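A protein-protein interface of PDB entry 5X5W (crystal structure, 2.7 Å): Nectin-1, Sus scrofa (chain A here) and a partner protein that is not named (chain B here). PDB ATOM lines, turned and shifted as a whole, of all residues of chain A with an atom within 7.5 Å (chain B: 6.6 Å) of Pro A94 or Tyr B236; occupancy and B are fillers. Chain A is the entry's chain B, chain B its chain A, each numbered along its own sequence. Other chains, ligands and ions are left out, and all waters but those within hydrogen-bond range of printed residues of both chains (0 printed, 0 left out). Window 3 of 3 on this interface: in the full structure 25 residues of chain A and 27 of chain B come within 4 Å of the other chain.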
ATOM      1  N   PRO A  22       4.467   8.614  -5.401  1.00  0.00           N
ATOM      2  CA  PRO A  22       3.333   7.827  -5.849  1.00  0.00           C
ATOM      3  C   PRO A  22       2.095   8.271  -5.091  1.00  0.00           C
ATOM      4  O   PRO A  22       2.084   8.205  -3.869  1.00  0.00           O
ATOM      5  CB  PRO A  22       3.750   6.433  -5.432  1.00  0.00           C
ATOM      6  CG  PRO A  22       4.391   6.640  -4.095  1.00  0.00           C
ATOM      7  CD  PRO A  22       4.782   8.077  -3.992  1.00  0.00           C
ATOM      8  N   GLY A  23       1.065   8.730  -5.783  1.00  0.00           N
ATOM      9  CA  GLY A  23       1.037   8.814  -7.222  1.00  0.00           C
ATOM     10  C   GLY A  23       0.678  10.210  -7.681  1.00  0.00           C
ATOM     11  O   GLY A  23      -0.430  10.455  -8.119  1.00  0.00           O
ATOM     12  N   VAL A  24       1.636  11.122  -7.592  1.00  0.00           N
ATOM     13  CA  VAL A  24       1.441  12.486  -8.015  1.00  0.00           C
ATOM     14  C   VAL A  24       1.732  12.642  -9.473  1.00  0.00           C
ATOM     15  O   VAL A  24       2.727  12.172  -9.947  1.00  0.00           O
ATOM     16  CB  VAL A  24       2.390  13.407  -7.274  1.00  0.00           C
ATOM     17  CG1 VAL A  24       2.121  13.324  -5.799  1.00  0.00           C
ATOM     18  CG2 VAL A  24       3.808  12.984  -7.547  1.00  0.00           C
ATOM     19  N   LYS A  25       0.861  13.328 -10.171  1.00  0.00           N
ATOM     20  CA  LYS A  25       1.083  13.649 -11.541  1.00  0.00           C
ATOM     21  C   LYS A  25       1.799  14.945 -11.444  1.00  0.00           C
ATOM     22  O   LYS A  25       1.505  15.721 -10.580  1.00  0.00           O
ATOM     23  CB  LYS A  25      -0.255  13.872 -12.204  1.00  0.00           C
ATOM     24  CG  LYS A  25      -0.245  13.846 -13.715  1.00  0.00           C
ATOM     25  CD  LYS A  25      -1.654  13.892 -14.281  1.00  0.00           C
ATOM     26  CE  LYS A  25      -1.791  14.977 -15.325  1.00  0.00           C
ATOM     27  NZ  LYS A  25      -3.149  15.032 -15.903  1.00  0.00           N
ATOM     28  N   THR A  92       1.551  20.027  -9.130  1.00  0.00           N
ATOM     29  CA  THR A  92       1.325  18.594  -8.940  1.00  0.00           C
ATOM     30  C   THR A  92      -0.116  18.289  -8.525  1.00  0.00           C
ATOM     31  O   THR A  92      -0.804  19.136  -7.952  1.00  0.00           O
ATOM     32  CB  THR A  92       2.290  17.999  -7.885  1.00  0.00           C
ATOM     33  OG1 THR A  92       2.066  18.616  -6.611  1.00  0.00           O
ATOM     34  CG2 THR A  92       3.728  18.224  -8.300  1.00  0.00           C
ATOM     35  N   PHE A  93      -0.559  17.072  -8.831  1.00  0.00           N
ATOM     36  CA  PHE A  93      -1.877  16.591  -8.437  1.00  0.00           C
ATOM     37  C   PHE A  93      -1.723  15.326  -7.615  1.00  0.00           C
ATOM     38  O   PHE A  93      -0.993  14.418  -8.007  1.00  0.00           O
ATOM     39  CB  PHE A  93      -2.758  16.308  -9.656  1.00  0.00           C
ATOM     40  CG  PHE A  93      -4.180  15.961  -9.306  1.00  0.00           C
ATOM     41  CD1 PHE A  93      -5.133  16.962  -9.174  1.00  0.00           C
ATOM     42  CD2 PHE A  93      -4.566  14.642  -9.110  1.00  0.00           C
ATOM     43  CE1 PHE A  93      -6.447  16.658  -8.854  1.00  0.00           C
ATOM     44  CE2 PHE A  93      -5.875  14.327  -8.790  1.00  0.00           C
ATOM     45  CZ  PHE A  93      -6.821  15.336  -8.661  1.00  0.00           C
ATOM     46  N   PRO A  94      -2.427  15.247  -6.479  1.00  0.00           N
ATOM     47  CA  PRO A  94      -3.347  16.260  -5.958  1.00  0.00           C
ATOM     48  C   PRO A  94      -2.703  17.180  -4.921  1.00  0.00           C
ATOM     49  O   PRO A  94      -3.416  17.852  -4.176  1.00  0.00           O
ATOM     50  CB  PRO A  94      -4.429  15.406  -5.308  1.00  0.00           C
ATOM     51  CG  PRO A  94      -3.632  14.249  -4.728  1.00  0.00           C
ATOM     52  CD  PRO A  94      -2.484  14.006  -5.685  1.00  0.00           C
ATOM     53  N   ALA A  95      -1.374  17.203  -4.876  1.00  0.00           N
ATOM     54  CA  ALA A  95      -0.641  17.895  -3.815  1.00  0.00           C
ATOM     55  C   ALA A  95      -0.602  19.414  -3.988  1.00  0.00           C
ATOM     56  O   ALA A  95      -0.334  20.144  -3.033  1.00  0.00           O
ATOM     57  CB  ALA A  95       0.776  17.346  -3.729  1.00  0.00           C
ATOM     58  N   GLY A  96      -0.858  19.883  -5.205  1.00  0.00           N
ATOM     59  CA  GLY A  96      -0.865  21.308  -5.485  1.00  0.00           C
ATOM     60  C   GLY A  96       0.492  21.858  -5.896  1.00  0.00           C
ATOM     61  O   GLY A  96       1.368  21.116  -6.343  1.00  0.00           O
ATOM     62  N   ASN A  97       0.666  23.169  -5.748  1.00  0.00           N
ATOM     63  CA  ASN A  97       1.926  23.809  -6.097  1.00  0.00           C
ATOM     64  C   ASN A  97       3.040  23.488  -5.119  1.00  0.00           C
ATOM     65  O   ASN A  97       2.915  23.708  -3.913  1.00  0.00           O
ATOM     66  CB  ASN A  97       1.760  25.321  -6.188  1.00  0.00           C
ATOM     67  CG  ASN A  97       1.020  25.744  -7.434  1.00  0.00           C
ATOM     68  OD1 ASN A  97       0.172  26.636  -7.395  1.00  0.00           O
ATOM     69  ND2 ASN A  97       1.326  25.096  -8.550  1.00  0.00           N
ATOM     70  N   ARG A  98       4.147  23.022  -5.684  1.00  0.00           N
ATOM     71  CA  ARG A  98       5.366  22.682  -4.979  1.00  0.00           C
ATOM     72  C   ARG A  98       6.513  23.437  -5.602  1.00  0.00           C
ATOM     73  O   ARG A  98       6.679  23.402  -6.793  1.00  0.00           O
ATOM     74  CB  ARG A  98       5.626  21.195  -5.145  1.00  0.00           C
ATOM     75  CG  ARG A  98       6.045  20.482  -3.885  1.00  0.00           C
ATOM     76  CD  ARG A  98       5.003  19.485  -3.431  1.00  0.00           C
ATOM     77  NE  ARG A  98       4.023  20.111  -2.557  1.00  0.00           N
ATOM     78  CZ  ARG A  98       3.594  19.604  -1.409  1.00  0.00           C
ATOM     79  NH1 ARG A  98       4.042  18.442  -0.968  1.00  0.00           N
ATOM     80  NH2 ARG A  98       2.701  20.263  -0.704  1.00  0.00           N
ATOM     81  N   PRO B  26      -7.536  10.098  -4.626  1.00  0.00           N
ATOM     82  CA  PRO B  26      -8.345  10.997  -5.461  1.00  0.00           C
ATOM     83  C   PRO B  26      -8.007  10.878  -6.944  1.00  0.00           C
ATOM     84  O   PRO B  26      -6.918  11.269  -7.362  1.00  0.00           O
ATOM     85  CB  PRO B  26      -7.984  12.385  -4.929  1.00  0.00           C
ATOM     86  CG  PRO B  26      -7.627  12.145  -3.504  1.00  0.00           C
ATOM     87  CD  PRO B  26      -6.944  10.800  -3.473  1.00  0.00           C
ATOM     88  N   TYR B 225      -5.084  24.441 -12.862  1.00  0.00           N
ATOM     89  CA  TYR B 225      -6.074  23.426 -13.201  1.00  0.00           C
ATOM     90  C   TYR B 225      -7.456  24.043 -13.404  1.00  0.00           C
ATOM     91  O   TYR B 225      -7.815  25.041 -12.770  1.00  0.00           O
ATOM     92  CB  TYR B 225      -6.155  22.347 -12.115  1.00  0.00           C
ATOM     93  CG  TYR B 225      -4.885  21.556 -11.887  1.00  0.00           C
ATOM     94  CD1 TYR B 225      -4.343  20.761 -12.889  1.00  0.00           C
ATOM     95  CD2 TYR B 225      -4.244  21.581 -10.654  1.00  0.00           C
ATOM     96  CE1 TYR B 225      -3.182  20.028 -12.674  1.00  0.00           C
ATOM     97  CE2 TYR B 225      -3.090  20.854 -10.428  1.00  0.00           C
ATOM     98  CZ  TYR B 225      -2.561  20.080 -11.441  1.00  0.00           C
ATOM     99  OH  TYR B 225      -1.409  19.359 -11.215  1.00  0.00           O
ATOM    100  N   PRO B 229     -10.436  19.725 -11.362  1.00  0.00           N
ATOM    101  CA  PRO B 229      -9.257  19.254 -10.623  1.00  0.00           C
ATOM    102  C   PRO B 229      -8.724  20.271  -9.612  1.00  0.00           C
ATOM    103  O   PRO B 229      -8.054  19.872  -8.663  1.00  0.00           O
ATOM    104  CB  PRO B 229      -8.230  18.984 -11.730  1.00  0.00           C
ATOM    105  CG  PRO B 229      -8.632  19.850 -12.837  1.00  0.00           C
ATOM    106  CD  PRO B 229     -10.128  19.942 -12.791  1.00  0.00           C
ATOM    107  N   ARG B 231     -10.532  21.893  -7.564  1.00  0.00           N
ATOM    108  CA  ARG B 231     -11.352  21.598  -6.408  1.00  0.00           C
ATOM    109  C   ARG B 231     -10.879  20.426  -5.618  1.00  0.00           C
ATOM    110  O   ARG B 231     -10.919  20.446  -4.416  1.00  0.00           O
ATOM    111  CB  ARG B 231     -12.742  21.285  -6.886  1.00  0.00           C
ATOM    112  CG  ARG B 231     -13.749  21.116  -5.794  1.00  0.00           C
ATOM    113  CD  ARG B 231     -14.688  19.968  -6.065  1.00  0.00           C
ATOM    114  NE  ARG B 231     -15.613  19.877  -4.962  1.00  0.00           N
ATOM    115  CZ  ARG B 231     -15.661  18.881  -4.097  1.00  0.00           C
ATOM    116  NH1 ARG B 231     -14.852  17.853  -4.215  1.00  0.00           N
ATOM    117  NH2 ARG B 231     -16.529  18.921  -3.115  1.00  0.00           N
ATOM    118  N   GLU B 232     -10.463  19.384  -6.305  1.00  0.00           N
ATOM    119  CA  GLU B 232      -9.941  18.186  -5.666  1.00  0.00           C
ATOM    120  C   GLU B 232      -8.632  18.463  -4.950  1.00  0.00           C
ATOM    121  O   GLU B 232      -8.359  17.871  -3.908  1.00  0.00           O
ATOM    122  CB  GLU B 232      -9.760  17.071  -6.688  1.00  0.00           C
ATOM    123  CG  GLU B 232     -11.082  16.479  -7.122  1.00  0.00           C
ATOM    124  CD  GLU B 232     -11.927  16.035  -5.931  1.00  0.00           C
ATOM    125  OE1 GLU B 232     -13.109  16.441  -5.840  1.00  0.00           O
ATOM    126  OE2 GLU B 232     -11.405  15.282  -5.080  1.00  0.00           O
ATOM    127  N   VAL B 233      -7.826  19.389  -5.432  1.00  0.00           N
ATOM    128  CA  VAL B 233      -6.609  19.697  -4.716  1.00  0.00           C
ATOM    129  C   VAL B 233      -6.854  20.546  -3.514  1.00  0.00           C
ATOM    130  O   VAL B 233      -6.279  20.324  -2.501  1.00  0.00           O
ATOM    131  CB  VAL B 233      -5.410  20.128  -5.605  1.00  0.00           C
ATOM    132  CG1 VAL B 233      -5.721  20.014  -7.052  1.00  0.00           C
ATOM    133  CG2 VAL B 233      -4.765  21.433  -5.235  1.00  0.00           C
ATOM    134  N   VAL B 234      -7.726  21.511  -3.615  1.00  0.00           N
ATOM    135  CA  VAL B 234      -8.045  22.296  -2.431  1.00  0.00           C
ATOM    136  C   VAL B 234      -8.773  21.435  -1.403  1.00  0.00           C
ATOM    137  O   VAL B 234      -8.555  21.567  -0.200  1.00  0.00           O
ATOM    138  CB  VAL B 234      -8.885  23.529  -2.806  1.00  0.00           C
ATOM    139  CG1 VAL B 234      -9.300  24.301  -1.562  1.00  0.00           C
ATOM    140  CG2 VAL B 234      -8.093  24.421  -3.756  1.00  0.00           C
ATOM    141  N   ASN B 235      -9.619  20.535  -1.893  1.00  0.00           N
ATOM    142  CA  ASN B 235     -10.332  19.603  -1.036  1.00  0.00           C
ATOM    143  C   ASN B 235      -9.390  18.642  -0.320  1.00  0.00           C
ATOM    144  O   ASN B 235      -9.614  18.301   0.837  1.00  0.00           O
ATOM    145  CB  ASN B 235     -11.351  18.810  -1.852  1.00  0.00           C
ATOM    146  CG  ASN B 235     -12.353  18.082  -0.981  1.00  0.00           C
ATOM    147  OD1 ASN B 235     -12.603  18.478   0.159  1.00  0.00           O
ATOM    148  ND2 ASN B 235     -12.938  17.016  -1.518  1.00  0.00           N
ATOM    149  N   TYR B 236      -8.342  18.208  -1.018  1.00  0.00           N
ATOM    150  CA  TYR B 236      -7.383  17.249  -0.475  1.00  0.00           C
ATOM    151  C   TYR B 236      -6.572  17.879   0.648  1.00  0.00           C
ATOM    152  O   TYR B 236      -6.246  17.227   1.633  1.00  0.00           O
ATOM    153  CB  TYR B 236      -6.472  16.733  -1.594  1.00  0.00           C
ATOM    154  CG  TYR B 236      -5.348  15.814  -1.166  1.00  0.00           C
ATOM    155  CD1 TYR B 236      -5.559  14.448  -0.984  1.00  0.00           C
ATOM    156  CD2 TYR B 236      -4.064  16.308  -0.975  1.00  0.00           C
ATOM    157  CE1 TYR B 236      -4.521  13.608  -0.600  1.00  0.00           C
ATOM    158  CE2 TYR B 236      -3.023  15.481  -0.596  1.00  0.00           C
ATOM    159  CZ  TYR B 236      -3.253  14.134  -0.411  1.00  0.00           C
ATOM    160  OH  TYR B 236      -2.203  13.328  -0.034  1.00  0.00           O
ATOM    161  N   TRP B 237      -6.255  19.157   0.502  1.00  0.00           N
ATOM    162  CA  TRP B 237      -5.542  19.887   1.540  1.00  0.00           C
ATOM    163  C   TRP B 237      -6.447  20.151   2.745  1.00  0.00           C
ATOM    164  O   TRP B 237      -6.058  19.909   3.889  1.00  0.00           O
ATOM    165  CB  TRP B 237      -4.999  21.203   0.985  1.00  0.00           C
ATOM    166  CG  TRP B 237      -4.614  22.164   2.046  1.00  0.00           C
ATOM    167  CD1 TRP B 237      -3.489  22.134   2.806  1.00  0.00           C
ATOM    168  CD2 TRP B 237      -5.358  23.306   2.473  1.00  0.00           C
ATOM    169  NE1 TRP B 237      -3.483  23.187   3.687  1.00  0.00           N
ATOM    170  CE2 TRP B 237      -4.623  23.922   3.501  1.00  0.00           C
ATOM    171  CE3 TRP B 237      -6.572  23.872   2.080  1.00  0.00           C
ATOM    172  CZ2 TRP B 237      -5.061  25.076   4.142  1.00  0.00           C
ATOM    173  CZ3 TRP B 237      -7.007  25.007   2.721  1.00  0.00           C
ATOM    174  CH2 TRP B 237      -6.252  25.597   3.742  1.00  0.00           C
ATOM    175  N   TYR B 238      -7.643  20.662   2.472  1.00  0.00           N
ATOM    176  CA  TYR B 238      -8.652  20.896   3.495  1.00  0.00           C
ATOM    177  C   TYR B 238      -8.846  19.622   4.318  1.00  0.00           C
ATOM    178  O   TYR B 238      -8.657  19.608   5.539  1.00  0.00           O
ATOM    179  CB  TYR B 238      -9.975  21.317   2.847  1.00  0.00           C
ATOM    180  CG  TYR B 238     -10.893  22.163   3.711  1.00  0.00           C
ATOM    181  CD1 TYR B 238     -12.280  22.104   3.551  1.00  0.00           C
ATOM    182  CD2 TYR B 238     -10.383  23.045   4.661  1.00  0.00           C
ATOM    183  CE1 TYR B 238     -13.125  22.875   4.323  1.00  0.00           C
ATOM    184  CE2 TYR B 238     -11.231  23.829   5.438  1.00  0.00           C
ATOM    185  CZ  TYR B 238     -12.597  23.739   5.260  1.00  0.00           C
ATOM    186  OH  TYR B 238     -13.444  24.513   6.025  1.00  0.00           O
ATOM    187  N   ARG B 239      -9.212  18.529   3.677  1.00  0.00           N
ATOM    188  CA  ARG B 239      -9.402  17.308   4.412  1.00  0.00           C
ATOM    189  C   ARG B 239      -8.225  17.029   5.261  1.00  0.00           C
ATOM    190  O   ARG B 239      -8.331  16.650   6.390  1.00  0.00           O
ATOM    191  CB  ARG B 239      -9.468  16.136   3.491  1.00  0.00           C
ATOM    192  CG  ARG B 239     -10.559  16.217   2.488  1.00  0.00           C
ATOM    193  CD  ARG B 239     -11.843  15.766   3.103  1.00  0.00           C
ATOM    194  NE  ARG B 239     -11.737  14.433   3.647  1.00  0.00           N
ATOM    195  CZ  ARG B 239     -12.789  13.714   3.973  1.00  0.00           C
ATOM    196  NH1 ARG B 239     -13.988  14.209   3.801  1.00  0.00           N
ATOM    197  NH2 ARG B 239     -12.654  12.512   4.450  1.00  0.00           N
ATOM    198  N   LYS B 240      -7.065  17.176   4.697  1.00  0.00           N
ATOM    199  CA  LYS B 240      -5.887  16.816   5.478  1.00  0.00           C
ATOM    200  C   LYS B 240      -5.817  17.654   6.765  1.00  0.00           C
ATOM    201  O   LYS B 240      -4.965  17.421   7.621  1.00  0.00           O
ATOM    202  CB  LYS B 240      -4.630  16.951   4.615  1.00  0.00           C
ATOM    203  CG  LYS B 240      -3.565  15.915   4.909  1.00  0.00           C
ATOM    204  CD  LYS B 240      -2.483  15.909   3.846  1.00  0.00           C
ATOM    205  CE  LYS B 240      -1.719  17.225   3.817  1.00  0.00           C
ATOM    206  NZ  LYS B 240      -0.569  17.186   2.860  1.00  0.00           N
ATOM    207  N   ASN B 241      -6.704  18.636   6.898  1.00  0.00           N
ATOM    208  CA  ASN B 241      -6.727  19.485   8.085  1.00  0.00           C
ATOM    209  C   ASN B 241      -8.027  19.297   8.881  1.00  0.00           C
ATOM    210  O   ASN B 241      -8.400  20.134   9.708  1.00  0.00           O
ATOM    211  CB  ASN B 241      -6.546  20.956   7.701  1.00  0.00           C
ATOM    212  CG  ASN B 241      -5.156  21.260   7.151  1.00  0.00           C
ATOM    213  OD1 ASN B 241      -4.228  21.563   7.905  1.00  0.00           O
ATOM    214  ND2 ASN B 241      -5.012  21.196   5.830  1.00  0.00           N
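Pro B26 touches Phe A93 (O to CE2, 3.5 Å). CE1 of Phe A93 touches O of Pro B229 (3.6 Å). CB of Glu B232 touches CZ of Phe A93, 3.9 Å away. Phe A93 touches Val B233 (CD1 to CG1, 3.8 Å). Pro A94 touches Val B233. Tyr B236 touches Pro A94 (CD2 to O, 3.6 Å). CG2 of Val B233 touches CA of Gly A96 (3.9 Å).
OH of Tyr B225 sits close to O of Thr A92, 3.3 Å away. N of Phe A93 sits at hydrogen-bond distance from OH of Tyr B225, 3.4 Å away.
O of Lys A25 lies within hydrogen-bond range of N of Phe A93 (3.0 Å). The backbone carbonyl oxygen (O) of Gly A96 lies within hydrogen-bond range of the side-chain hydroxyl (OG1) of Thr A92 (2.6 Å). The side-chain carboxylate of Glu B232 is in salt-bridge range of the guanidinium group of Arg B231 (2.8 Å).
Val A24 touches none of the printed residues of chain B. Printed residues of chain B within 4 Å of Thr A92: Tyr B225 (3.2 Å). Of chain B, only Val B233 and Tyr B236 come within 4 Å of Pro A94. Printed residues of chain B within 4 Å of Gly A96: Val B233. Of the printed residues of chain A, Pro B229 touches Phe A93. Of the printed residues of chain A, Val B233 touches Phe A93, Pro A94 and Gly A96. Val B234 touches none of the printed residues of chain A. Of chain A, only Pro A94 (3.6 Å) comes within 4 Å of Tyr B236. The nearest residue of chain B that does not touch Pro A94 is Pro B26 (4.7 Å). The nearest residue of chain A that does not touch Tyr B236 is Ala A95 (4.7 Å).
Hydrophobic or aromatic side chains of chain A within 4 Å of the printed part of chain B: Phe A93. Of the 14 printed residues of chain B, 6 touch a printed residue of chain A.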
